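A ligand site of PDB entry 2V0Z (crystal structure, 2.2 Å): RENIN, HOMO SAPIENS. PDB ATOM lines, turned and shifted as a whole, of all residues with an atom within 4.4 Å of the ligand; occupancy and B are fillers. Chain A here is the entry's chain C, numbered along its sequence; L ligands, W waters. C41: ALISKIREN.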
ATOM      1  N   THR A  18      24.584   2.946  27.909  1.00  0.00           N
ATOM      2  CA  THR A  18      23.919   4.233  27.954  1.00  0.00           C
ATOM      3  C   THR A  18      23.067   4.528  26.724  1.00  0.00           C
ATOM      4  O   THR A  18      22.194   5.398  26.781  1.00  0.00           O
ATOM      5  CB  THR A  18      24.917   5.402  28.185  1.00  0.00           C
ATOM      6  OG1 THR A  18      25.924   5.387  27.168  1.00  0.00           O
ATOM      7  CG2 THR A  18      25.591   5.286  29.551  1.00  0.00           C
ATOM      8  N   GLN A  19      23.337   3.847  25.618  1.00  0.00           N
ATOM      9  CA  GLN A  19      22.571   4.070  24.403  1.00  0.00           C
ATOM     10  C   GLN A  19      22.133   2.754  23.803  1.00  0.00           C
ATOM     11  O   GLN A  19      22.962   1.899  23.499  1.00  0.00           O
ATOM     12  CB  GLN A  19      23.395   4.851  23.368  1.00  0.00           C
ATOM     13  CG  GLN A  19      23.720   6.238  23.841  1.00  0.00           C
ATOM     14  CD  GLN A  19      24.585   6.966  22.881  1.00  0.00           C
ATOM     15  OE1 GLN A  19      25.523   7.676  23.278  1.00  0.00           O
ATOM     16  NE2 GLN A  19      24.298   6.817  21.598  1.00  0.00           N
ATOM     17  N   TYR A  20      20.819   2.572  23.680  1.00  0.00           N
ATOM     18  CA  TYR A  20      20.268   1.362  23.094  1.00  0.00           C
ATOM     19  C   TYR A  20      19.527   1.765  21.843  1.00  0.00           C
ATOM     20  O   TYR A  20      18.636   2.623  21.894  1.00  0.00           O
ATOM     21  CB  TYR A  20      19.332   0.655  24.062  1.00  0.00           C
ATOM     22  CG  TYR A  20      20.040   0.050  25.257  1.00  0.00           C
ATOM     23  CD1 TYR A  20      20.388   0.844  26.346  1.00  0.00           C
ATOM     24  CD2 TYR A  20      20.300  -1.333  25.327  1.00  0.00           C
ATOM     25  CE1 TYR A  20      20.976   0.291  27.479  1.00  0.00           C
ATOM     26  CE2 TYR A  20      20.887  -1.886  26.461  1.00  0.00           C
ATOM     27  CZ  TYR A  20      21.218  -1.060  27.538  1.00  0.00           C
ATOM     28  OH  TYR A  20      21.753  -1.580  28.684  1.00  0.00           O
ATOM     29  N   VAL A  36      16.891   5.183  18.178  1.00  0.00           N
ATOM     30  CA  VAL A  36      16.486   4.903  19.558  1.00  0.00           C
ATOM     31  C   VAL A  36      14.966   4.790  19.496  1.00  0.00           C
ATOM     32  O   VAL A  36      14.333   5.582  18.797  1.00  0.00           O
ATOM     33  CB  VAL A  36      16.828   6.095  20.507  1.00  0.00           C
ATOM     34  CG1 VAL A  36      16.242   5.882  21.904  1.00  0.00           C
ATOM     35  CG2 VAL A  36      18.330   6.290  20.598  1.00  0.00           C
ATOM     36  N   ASP A  38      12.183   5.434  21.432  1.00  0.00           N
ATOM     37  CA  ASP A  38      11.957   6.291  22.578  1.00  0.00           C
ATOM     38  C   ASP A  38      10.528   6.465  23.059  1.00  0.00           C
ATOM     39  O   ASP A  38       9.764   7.252  22.482  1.00  0.00           O
ATOM     40  CB  ASP A  38      12.569   7.642  22.186  1.00  0.00           C
ATOM     41  CG  ASP A  38      12.387   8.703  23.214  1.00  0.00           C
ATOM     42  OD1 ASP A  38      12.508   8.407  24.425  1.00  0.00           O
ATOM     43  OD2 ASP A  38      12.144   9.859  22.817  1.00  0.00           O
ATOM     44  N   GLY A  40       9.689   8.108  25.384  1.00  0.00           N
ATOM     45  CA  GLY A  40       9.599   9.459  25.905  1.00  0.00           C
ATOM     46  C   GLY A  40       9.033  10.464  24.912  1.00  0.00           C
ATOM     47  O   GLY A  40       8.719  11.571  25.313  1.00  0.00           O
ATOM     48  N   SER A  41       8.933  10.116  23.621  1.00  0.00           N
ATOM     49  CA  SER A  41       8.405  11.038  22.608  1.00  0.00           C
ATOM     50  C   SER A  41       7.598  10.273  21.555  1.00  0.00           C
ATOM     51  O   SER A  41       7.584   9.043  21.579  1.00  0.00           O
ATOM     52  CB  SER A  41       9.533  11.824  21.943  1.00  0.00           C
ATOM     53  OG  SER A  41      10.421  10.967  21.266  1.00  0.00           O
ATOM     54  N   ARG A  82      11.659  19.528  20.768  1.00  0.00           N
ATOM     55  CA  ARG A  82      12.360  19.912  21.970  1.00  0.00           C
ATOM     56  C   ARG A  82      12.343  18.825  23.037  1.00  0.00           C
ATOM     57  O   ARG A  82      11.307  18.599  23.676  1.00  0.00           O
ATOM     58  CB  ARG A  82      11.765  21.203  22.527  1.00  0.00           C
ATOM     59  CG  ARG A  82      12.109  22.421  21.693  1.00  0.00           C
ATOM     60  CD  ARG A  82      11.221  23.609  22.014  1.00  0.00           C
ATOM     61  NE  ARG A  82      10.581  24.104  20.792  1.00  0.00           N
ATOM     62  CZ  ARG A  82      10.536  25.390  20.423  1.00  0.00           C
ATOM     63  NH1 ARG A  82      11.088  26.327  21.191  1.00  0.00           N
ATOM     64  NH2 ARG A  82       9.945  25.721  19.274  1.00  0.00           N
ATOM     65  N   TYR A  83      13.463  18.128  23.220  1.00  0.00           N
ATOM     66  CA  TYR A  83      13.572  17.081  24.233  1.00  0.00           C
ATOM     67  C   TYR A  83      14.214  17.720  25.445  1.00  0.00           C
ATOM     68  O   TYR A  83      14.883  18.762  25.332  1.00  0.00           O
ATOM     69  CB  TYR A  83      14.443  15.931  23.754  1.00  0.00           C
ATOM     70  CG  TYR A  83      13.972  15.310  22.465  1.00  0.00           C
ATOM     71  CD1 TYR A  83      12.909  14.414  22.449  1.00  0.00           C
ATOM     72  CD2 TYR A  83      14.598  15.620  21.264  1.00  0.00           C
ATOM     73  CE1 TYR A  83      12.494  13.823  21.257  1.00  0.00           C
ATOM     74  CE2 TYR A  83      14.174  15.040  20.061  1.00  0.00           C
ATOM     75  CZ  TYR A  83      13.142  14.142  20.075  1.00  0.00           C
ATOM     76  OH  TYR A  83      12.808  13.512  18.905  1.00  0.00           O
ATOM     77  N   SER A  84      14.063  17.090  26.604  1.00  0.00           N
ATOM     78  CA  SER A  84      14.654  17.633  27.824  1.00  0.00           C
ATOM     79  C   SER A  84      16.167  17.878  27.781  1.00  0.00           C
ATOM     80  O   SER A  84      16.687  18.632  28.578  1.00  0.00           O
ATOM     81  CB  SER A  84      14.304  16.748  29.034  1.00  0.00           C
ATOM     82  OG  SER A  84      14.844  15.440  28.935  1.00  0.00           O
ATOM     83  N   THR A  85      16.881  17.254  26.855  1.00  0.00           N
ATOM     84  CA  THR A  85      18.317  17.460  26.824  1.00  0.00           C
ATOM     85  C   THR A  85      18.867  17.951  25.494  1.00  0.00           C
ATOM     86  O   THR A  85      20.081  17.950  25.291  1.00  0.00           O
ATOM     87  CB  THR A  85      19.079  16.171  27.229  1.00  0.00           C
ATOM     88  OG1 THR A  85      18.580  15.058  26.471  1.00  0.00           O
ATOM     89  CG2 THR A  85      18.946  15.886  28.747  1.00  0.00           C
ATOM     90  N   PRO A 118      23.609  17.339  22.312  1.00  0.00           N
ATOM     91  CA  PRO A 118      24.299  16.075  22.549  1.00  0.00           C
ATOM     92  C   PRO A 118      24.551  15.156  21.339  1.00  0.00           C
ATOM     93  O   PRO A 118      25.216  14.137  21.483  1.00  0.00           O
ATOM     94  CB  PRO A 118      23.337  15.385  23.489  1.00  0.00           C
ATOM     95  CG  PRO A 118      21.988  15.727  22.829  1.00  0.00           C
ATOM     96  CD  PRO A 118      22.144  17.178  22.435  1.00  0.00           C
ATOM     97  N   LEU A 121      27.640  13.117  20.471  1.00  0.00           N
ATOM     98  CA  LEU A 121      27.898  12.037  21.424  1.00  0.00           C
ATOM     99  C   LEU A 121      26.961  10.848  21.196  1.00  0.00           C
ATOM    100  O   LEU A 121      27.063   9.829  21.866  1.00  0.00           O
ATOM    101  CB  LEU A 121      27.766  12.529  22.865  1.00  0.00           C
ATOM    102  CG  LEU A 121      28.717  13.666  23.280  1.00  0.00           C
ATOM    103  CD1 LEU A 121      28.332  14.168  24.639  1.00  0.00           C
ATOM    104  CD2 LEU A 121      30.150  13.195  23.310  1.00  0.00           C
ATOM    105  N   ALA A 122      26.095  10.972  20.194  1.00  0.00           N
ATOM    106  CA  ALA A 122      25.143   9.925  19.850  1.00  0.00           C
ATOM    107  C   ALA A 122      25.717   8.873  18.894  1.00  0.00           C
ATOM    108  O   ALA A 122      26.355   9.187  17.870  1.00  0.00           O
ATOM    109  CB  ALA A 122      23.864  10.544  19.230  1.00  0.00           C
ATOM    110  N   PHE A 124      23.577   6.696  17.796  1.00  0.00           N
ATOM    111  CA  PHE A 124      22.415   6.557  16.913  1.00  0.00           C
ATOM    112  C   PHE A 124      22.341   7.751  15.996  1.00  0.00           C
ATOM    113  O   PHE A 124      22.916   8.807  16.290  1.00  0.00           O
ATOM    114  CB  PHE A 124      21.109   6.459  17.738  1.00  0.00           C
ATOM    115  CG  PHE A 124      20.922   7.578  18.742  1.00  0.00           C
ATOM    116  CD1 PHE A 124      20.141   8.698  18.425  1.00  0.00           C
ATOM    117  CD2 PHE A 124      21.501   7.503  20.022  1.00  0.00           C
ATOM    118  CE1 PHE A 124      19.922   9.741  19.392  1.00  0.00           C
ATOM    119  CE2 PHE A 124      21.292   8.520  20.973  1.00  0.00           C
ATOM    120  CZ  PHE A 124      20.494   9.639  20.660  1.00  0.00           C
ATOM    121  N   VAL A 127      15.626   8.919  15.774  1.00  0.00           N
ATOM    122  CA  VAL A 127      14.691   8.489  16.813  1.00  0.00           C
ATOM    123  C   VAL A 127      13.384   7.966  16.238  1.00  0.00           C
ATOM    124  O   VAL A 127      12.921   8.432  15.196  1.00  0.00           O
ATOM    125  CB  VAL A 127      14.321   9.736  17.742  1.00  0.00           C
ATOM    126  CG1 VAL A 127      13.270   9.374  18.818  1.00  0.00           C
ATOM    127  CG2 VAL A 127      15.589  10.325  18.378  1.00  0.00           C
ATOM    128  N   GLN A 135       1.367  13.297  22.227  1.00  0.00           N
ATOM    129  CA  GLN A 135       2.662  13.950  22.430  1.00  0.00           C
ATOM    130  C   GLN A 135       3.436  14.225  21.139  1.00  0.00           C
ATOM    131  O   GLN A 135       4.536  14.797  21.174  1.00  0.00           O
ATOM    132  CB  GLN A 135       3.515  13.129  23.387  1.00  0.00           C
ATOM    133  CG  GLN A 135       2.883  12.969  24.761  1.00  0.00           C
ATOM    134  CD  GLN A 135       2.702  14.305  25.444  1.00  0.00           C
ATOM    135  OE1 GLN A 135       3.656  15.071  25.602  1.00  0.00           O
ATOM    136  NE2 GLN A 135       1.482  14.605  25.845  1.00  0.00           N
ATOM    137  N   ILE A 137       4.613  16.024  17.989  1.00  0.00           N
ATOM    138  CA  ILE A 137       4.723  17.401  17.525  1.00  0.00           C
ATOM    139  C   ILE A 137       4.146  17.403  16.102  1.00  0.00           C
ATOM    140  O   ILE A 137       4.393  16.481  15.317  1.00  0.00           O
ATOM    141  CB  ILE A 137       6.207  17.900  17.520  1.00  0.00           C
ATOM    142  CG1 ILE A 137       6.841  17.780  18.917  1.00  0.00           C
ATOM    143  CG2 ILE A 137       6.302  19.321  16.986  1.00  0.00           C
ATOM    144  CD1 ILE A 137       6.106  18.505  20.011  1.00  0.00           C
ATOM    145  N   TYR A 162      16.526  -4.740  27.727  1.00  0.00           N
ATOM    146  CA  TYR A 162      17.841  -4.098  27.639  1.00  0.00           C
ATOM    147  C   TYR A 162      18.833  -4.968  28.393  1.00  0.00           C
ATOM    148  O   TYR A 162      18.660  -5.217  29.586  1.00  0.00           O
ATOM    149  CB  TYR A 162      17.844  -2.692  28.266  1.00  0.00           C
ATOM    150  CG  TYR A 162      17.252  -1.620  27.383  1.00  0.00           C
ATOM    151  CD1 TYR A 162      16.868  -1.889  26.078  1.00  0.00           C
ATOM    152  CD2 TYR A 162      17.060  -0.329  27.858  1.00  0.00           C
ATOM    153  CE1 TYR A 162      16.309  -0.897  25.259  1.00  0.00           C
ATOM    154  CE2 TYR A 162      16.499   0.668  27.056  1.00  0.00           C
ATOM    155  CZ  TYR A 162      16.126   0.376  25.765  1.00  0.00           C
ATOM    156  OH  TYR A 162      15.612   1.371  24.958  1.00  0.00           O
ATOM    157  N   LEU A 224       7.905   8.536  34.616  1.00  0.00           N
ATOM    158  CA  LEU A 224       7.706   8.365  33.194  1.00  0.00           C
ATOM    159  C   LEU A 224       8.674   7.228  32.803  1.00  0.00           C
ATOM    160  O   LEU A 224       9.852   7.298  33.139  1.00  0.00           O
ATOM    161  CB  LEU A 224       8.035   9.678  32.458  1.00  0.00           C
ATOM    162  CG  LEU A 224       7.450   9.826  31.053  1.00  0.00           C
ATOM    163  CD1 LEU A 224       7.449  11.271  30.669  1.00  0.00           C
ATOM    164  CD2 LEU A 224       8.226   9.024  30.030  1.00  0.00           C
ATOM    165  N   ASP A 226      10.860   5.819  30.439  1.00  0.00           N
ATOM    166  CA  ASP A 226      11.525   6.283  29.230  1.00  0.00           C
ATOM    167  C   ASP A 226      12.582   5.342  28.656  1.00  0.00           C
ATOM    168  O   ASP A 226      13.736   5.332  29.108  1.00  0.00           O
ATOM    169  CB  ASP A 226      12.132   7.662  29.539  1.00  0.00           C
ATOM    170  CG  ASP A 226      12.624   8.403  28.299  1.00  0.00           C
ATOM    171  OD1 ASP A 226      13.114   9.539  28.461  1.00  0.00           O
ATOM    172  OD2 ASP A 226      12.525   7.882  27.173  1.00  0.00           O
ATOM    173  N   THR A 227      12.250   4.631  27.588  1.00  0.00           N
ATOM    174  CA  THR A 227      13.184   3.712  26.954  1.00  0.00           C
ATOM    175  C   THR A 227      14.334   4.466  26.247  1.00  0.00           C
ATOM    176  O   THR A 227      15.396   3.901  25.966  1.00  0.00           O
ATOM    177  CB  THR A 227      12.458   2.841  25.955  1.00  0.00           C
ATOM    178  OG1 THR A 227      11.759   3.679  25.021  1.00  0.00           O
ATOM    179  CG2 THR A 227      11.437   1.942  26.680  1.00  0.00           C
ATOM    180  N   GLY A 228      14.115   5.752  25.967  1.00  0.00           N
ATOM    181  CA  GLY A 228      15.131   6.553  25.312  1.00  0.00           C
ATOM    182  C   GLY A 228      15.987   7.362  26.287  1.00  0.00           C
ATOM    183  O   GLY A 228      16.611   8.349  25.898  1.00  0.00           O
ATOM    184  N   ALA A 229      16.007   6.950  27.560  1.00  0.00           N
ATOM    185  CA  ALA A 229      16.785   7.636  28.589  1.00  0.00           C
ATOM    186  C   ALA A 229      17.836   6.667  29.113  1.00  0.00           C
ATOM    187  O   ALA A 229      17.545   5.496  29.317  1.00  0.00           O
ATOM    188  CB  ALA A 229      15.873   8.068  29.742  1.00  0.00           C
ATOM    189  N   SER A 230      19.055   7.159  29.339  1.00  0.00           N
ATOM    190  CA  SER A 230      20.119   6.318  29.835  1.00  0.00           C
ATOM    191  C   SER A 230      19.970   6.001  31.305  1.00  0.00           C
ATOM    192  O   SER A 230      20.245   4.887  31.725  1.00  0.00           O
ATOM    193  CB  SER A 230      21.498   6.968  29.620  1.00  0.00           C
ATOM    194  OG  SER A 230      21.619   7.508  28.330  1.00  0.00           O
ATOM    195  N   ILE A 305      11.775  18.077  34.362  1.00  0.00           N
ATOM    196  CA  ILE A 305      10.895  18.145  33.211  1.00  0.00           C
ATOM    197  C   ILE A 305       9.796  19.137  33.583  1.00  0.00           C
ATOM    198  O   ILE A 305       9.225  19.062  34.669  1.00  0.00           O
ATOM    199  CB  ILE A 305      10.303  16.730  32.854  1.00  0.00           C
ATOM    200  CG1 ILE A 305      11.391  15.838  32.252  1.00  0.00           C
ATOM    201  CG2 ILE A 305       9.166  16.838  31.837  1.00  0.00           C
ATOM    202  CD1 ILE A 305      12.134  15.045  33.258  1.00  0.00           C
ATOM    203  N   THR A 309       3.977  17.655  31.526  1.00  0.00           N
ATOM    204  CA  THR A 309       4.470  16.298  31.779  1.00  0.00           C
ATOM    205  C   THR A 309       5.176  16.241  33.127  1.00  0.00           C
ATOM    206  O   THR A 309       4.883  15.377  33.939  1.00  0.00           O
ATOM    207  CB  THR A 309       5.414  15.818  30.645  1.00  0.00           C
ATOM    208  OG1 THR A 309       4.676  15.802  29.417  1.00  0.00           O
ATOM    209  CG2 THR A 309       5.922  14.411  30.921  1.00  0.00           C
ATOM    210  N   ALA A 317      17.072   3.289  31.156  1.00  0.00           N
ATOM    211  CA  ALA A 317      17.809   2.039  31.026  1.00  0.00           C
ATOM    212  C   ALA A 317      18.315   1.450  32.352  1.00  0.00           C
ATOM    213  O   ALA A 317      18.393   0.241  32.467  1.00  0.00           O
ATOM    214  CB  ALA A 317      18.947   2.189  30.017  1.00  0.00           C
HETATM  215  C1  C41 L   1      18.579   4.273  26.269  1.00  0.00           C
HETATM  216  O2  C41 L   1      19.411   4.741  25.234  1.00  0.00           O
HETATM  217  C3  C41 L   1      18.657   5.683  24.426  1.00  0.00           C
HETATM  218  C4  C41 L   1      19.509   6.911  24.073  1.00  0.00           C
HETATM  219  C5  C41 L   1      20.135   7.518  25.334  1.00  0.00           C
HETATM  220  O6  C41 L   1      21.027   8.601  25.023  1.00  0.00           O
HETATM  221  C7  C41 L   1      20.512   9.847  24.641  1.00  0.00           C
HETATM  222  C8  C41 L   1      19.200  10.227  24.836  1.00  0.00           C
HETATM  223  C9  C41 L   1      18.794  11.486  24.369  1.00  0.00           C
HETATM  224  C10 C41 L   1      19.723  12.350  23.719  1.00  0.00           C
HETATM  225  C11 C41 L   1      21.037  11.980  23.533  1.00  0.00           C
HETATM  226  C12 C41 L   1      21.431  10.713  24.001  1.00  0.00           C
HETATM  227  O13 C41 L   1      22.766  10.203  23.907  1.00  0.00           O
HETATM  228  C14 C41 L   1      23.790  10.983  23.253  1.00  0.00           C
HETATM  229  C15 C41 L   1      17.349  11.939  24.554  1.00  0.00           C
HETATM  230  C16 C41 L   1      16.323  10.974  23.934  1.00  0.00           C
HETATM  231  C17 C41 L   1      16.657  10.699  22.441  1.00  0.00           C
HETATM  232  C18 C41 L   1      15.761   9.590  21.869  1.00  0.00           C
HETATM  233  C19 C41 L   1      16.578  11.996  21.591  1.00  0.00           C
HETATM  234  C20 C41 L   1      14.923  11.582  24.088  1.00  0.00           C
HETATM  235  C21 C41 L   1      14.380  11.612  25.524  1.00  0.00           C
HETATM  236  N22 C41 L   1      14.266  10.220  26.016  1.00  0.00           N
HETATM  237  C23 C41 L   1      13.005  12.300  25.561  1.00  0.00           C
HETATM  238  O24 C41 L   1      12.029  11.398  25.045  1.00  0.00           O
HETATM  239  C25 C41 L   1      12.588  12.661  27.011  1.00  0.00           C
HETATM  240  C26 C41 L   1      11.163  13.263  27.133  1.00  0.00           C
HETATM  241  C27 C41 L   1      10.856  13.779  28.572  1.00  0.00           C
HETATM  242  C28 C41 L   1       9.405  14.307  28.663  1.00  0.00           C
HETATM  243  C29 C41 L   1      11.071  12.673  29.605  1.00  0.00           C
HETATM  244  C30 C41 L   1      11.016  14.400  26.119  1.00  0.00           C
HETATM  245  O31 C41 L   1      11.753  15.400  26.173  1.00  0.00           O
HETATM  246  N32 C41 L   1      10.096  14.216  25.186  1.00  0.00           N
HETATM  247  C33 C41 L   1       9.838  15.154  24.092  1.00  0.00           C
HETATM  248  C34 C41 L   1       8.427  15.736  24.094  1.00  0.00           C
HETATM  249  C35 C41 L   1       7.367  14.636  23.999  1.00  0.00           C
HETATM  250  C36 C41 L   1       8.317  16.638  22.880  1.00  0.00           C
HETATM  251  C37 C41 L   1       8.300  16.542  25.264  1.00  0.00           C
HETATM  252  O38 C41 L   1       7.480  16.208  26.122  1.00  0.00           O
HETATM  253  N39 C41 L   1       9.127  17.566  25.427  1.00  0.00           N
HETATM  254  O   HOH W   1       5.592  14.431  27.158  1.00  0.00           O
HETATM  255  O   HOH W   2      16.113  13.960  27.188  1.00  0.00           O
HETATM  256  O   HOH W   3      23.304   9.256  26.916  1.00  0.00           O
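OD1 of Asp 38 sits close to N of Gly 40, 3.0 Å away. The backbone NH (N) of Gly 228 sits close to the side-chain carboxylate (OD1) of Asp 38, at 3.5 Å. OD2 of Asp 38 is in hydrogen-bond range of OG of Ser 41, at 2.6 Å. The side-chain carboxylate (OD2) of Asp 226 is in hydrogen-bond range of the backbone NH (N) of Gly 40. The side-chain carboxylate (OD2) of Asp 226 lies within hydrogen-bond range of the backbone NH (N) of Gly 228 (2.9 Å). The backbone carbonyl oxygen of Thr 227 sits at hydrogen-bond distance from the side-chain hydroxyl of Tyr 162 (2.7 Å). The backbone carbonyl oxygen of Thr 18 sits at hydrogen-bond distance from the side-chain hydroxyl of Ser 230, at 2.7 Å. The backbone carbonyl oxygen (O) of Ala 229 is in hydrogen-bond range of the backbone NH (N) of Ala 317 (2.9 Å).
Water W1 lies within hydrogen-bond range of the side-chain amide oxygen (OE1) of Gln 135, an oxygen (O38) of the ligand and the side-chain hydroxyl (OG1) of Thr 309. Water W3 lies within hydrogen-bond range of OG of Ser 230 and O6 of the ligand. Water W2 bridges the side-chain hydroxyl (OG) of Ser 84 (2.6 Å) and the side-chain hydroxyl (OG1) of Thr 85 (2.8 Å).
The side-chain carboxylate (OD1) of Asp 38 lies within salt-bridge range of a nitrogen (N22) of the ligand, 3.0 Å away. The side-chain carboxylate of Asp 226 lies within salt-bridge range of a nitrogen (N22) of the ligand (2.8 Å). The backbone NH (N) of Ser 84 sits at hydrogen-bond distance from an oxygen (O31) of the ligand, 2.9 Å away. N39 of the ligand sits at hydrogen-bond distance from O of Arg 82. A nitrogen (N32) of the ligand sits at hydrogen-bond distance from the backbone carbonyl oxygen (O) of Gly 40, at 3.0 Å. N22 of the ligand lies within hydrogen-bond range of O of Gly 228 (3.0 Å). N of Tyr 20 lies within hydrogen-bond range of O2 of the ligand (3.0 Å).
An oxygen (O2) of the ligand sits close to the backbone carbonyl oxygen (O) of Thr 18 (3.3 Å). Gln 19 touches the ligand. CG1 of Val 36 touches C3 of the ligand (3.5 Å). N of Ser 41 touches O24 of the ligand (3.6 Å). CA of Tyr 83 touches O31 of the ligand, at 3.1 Å. Thr 85 touches the ligand. O of Pro 118 touches C14 of the ligand, at 3.9 Å. O of Leu 121 touches C14 of the ligand, at 3.7 Å. Ala 122 touches the ligand. CZ of Phe 124 touches C12 of the ligand, 3.6 Å away. Val 127 touches the ligand. Thr 227 touches the ligand (O to C1, 3.2 Å). Ala 229 touches the ligand. Ser 230 touches the ligand. Of the 28 residues printed, 21 come within 4 Å of the ligand.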
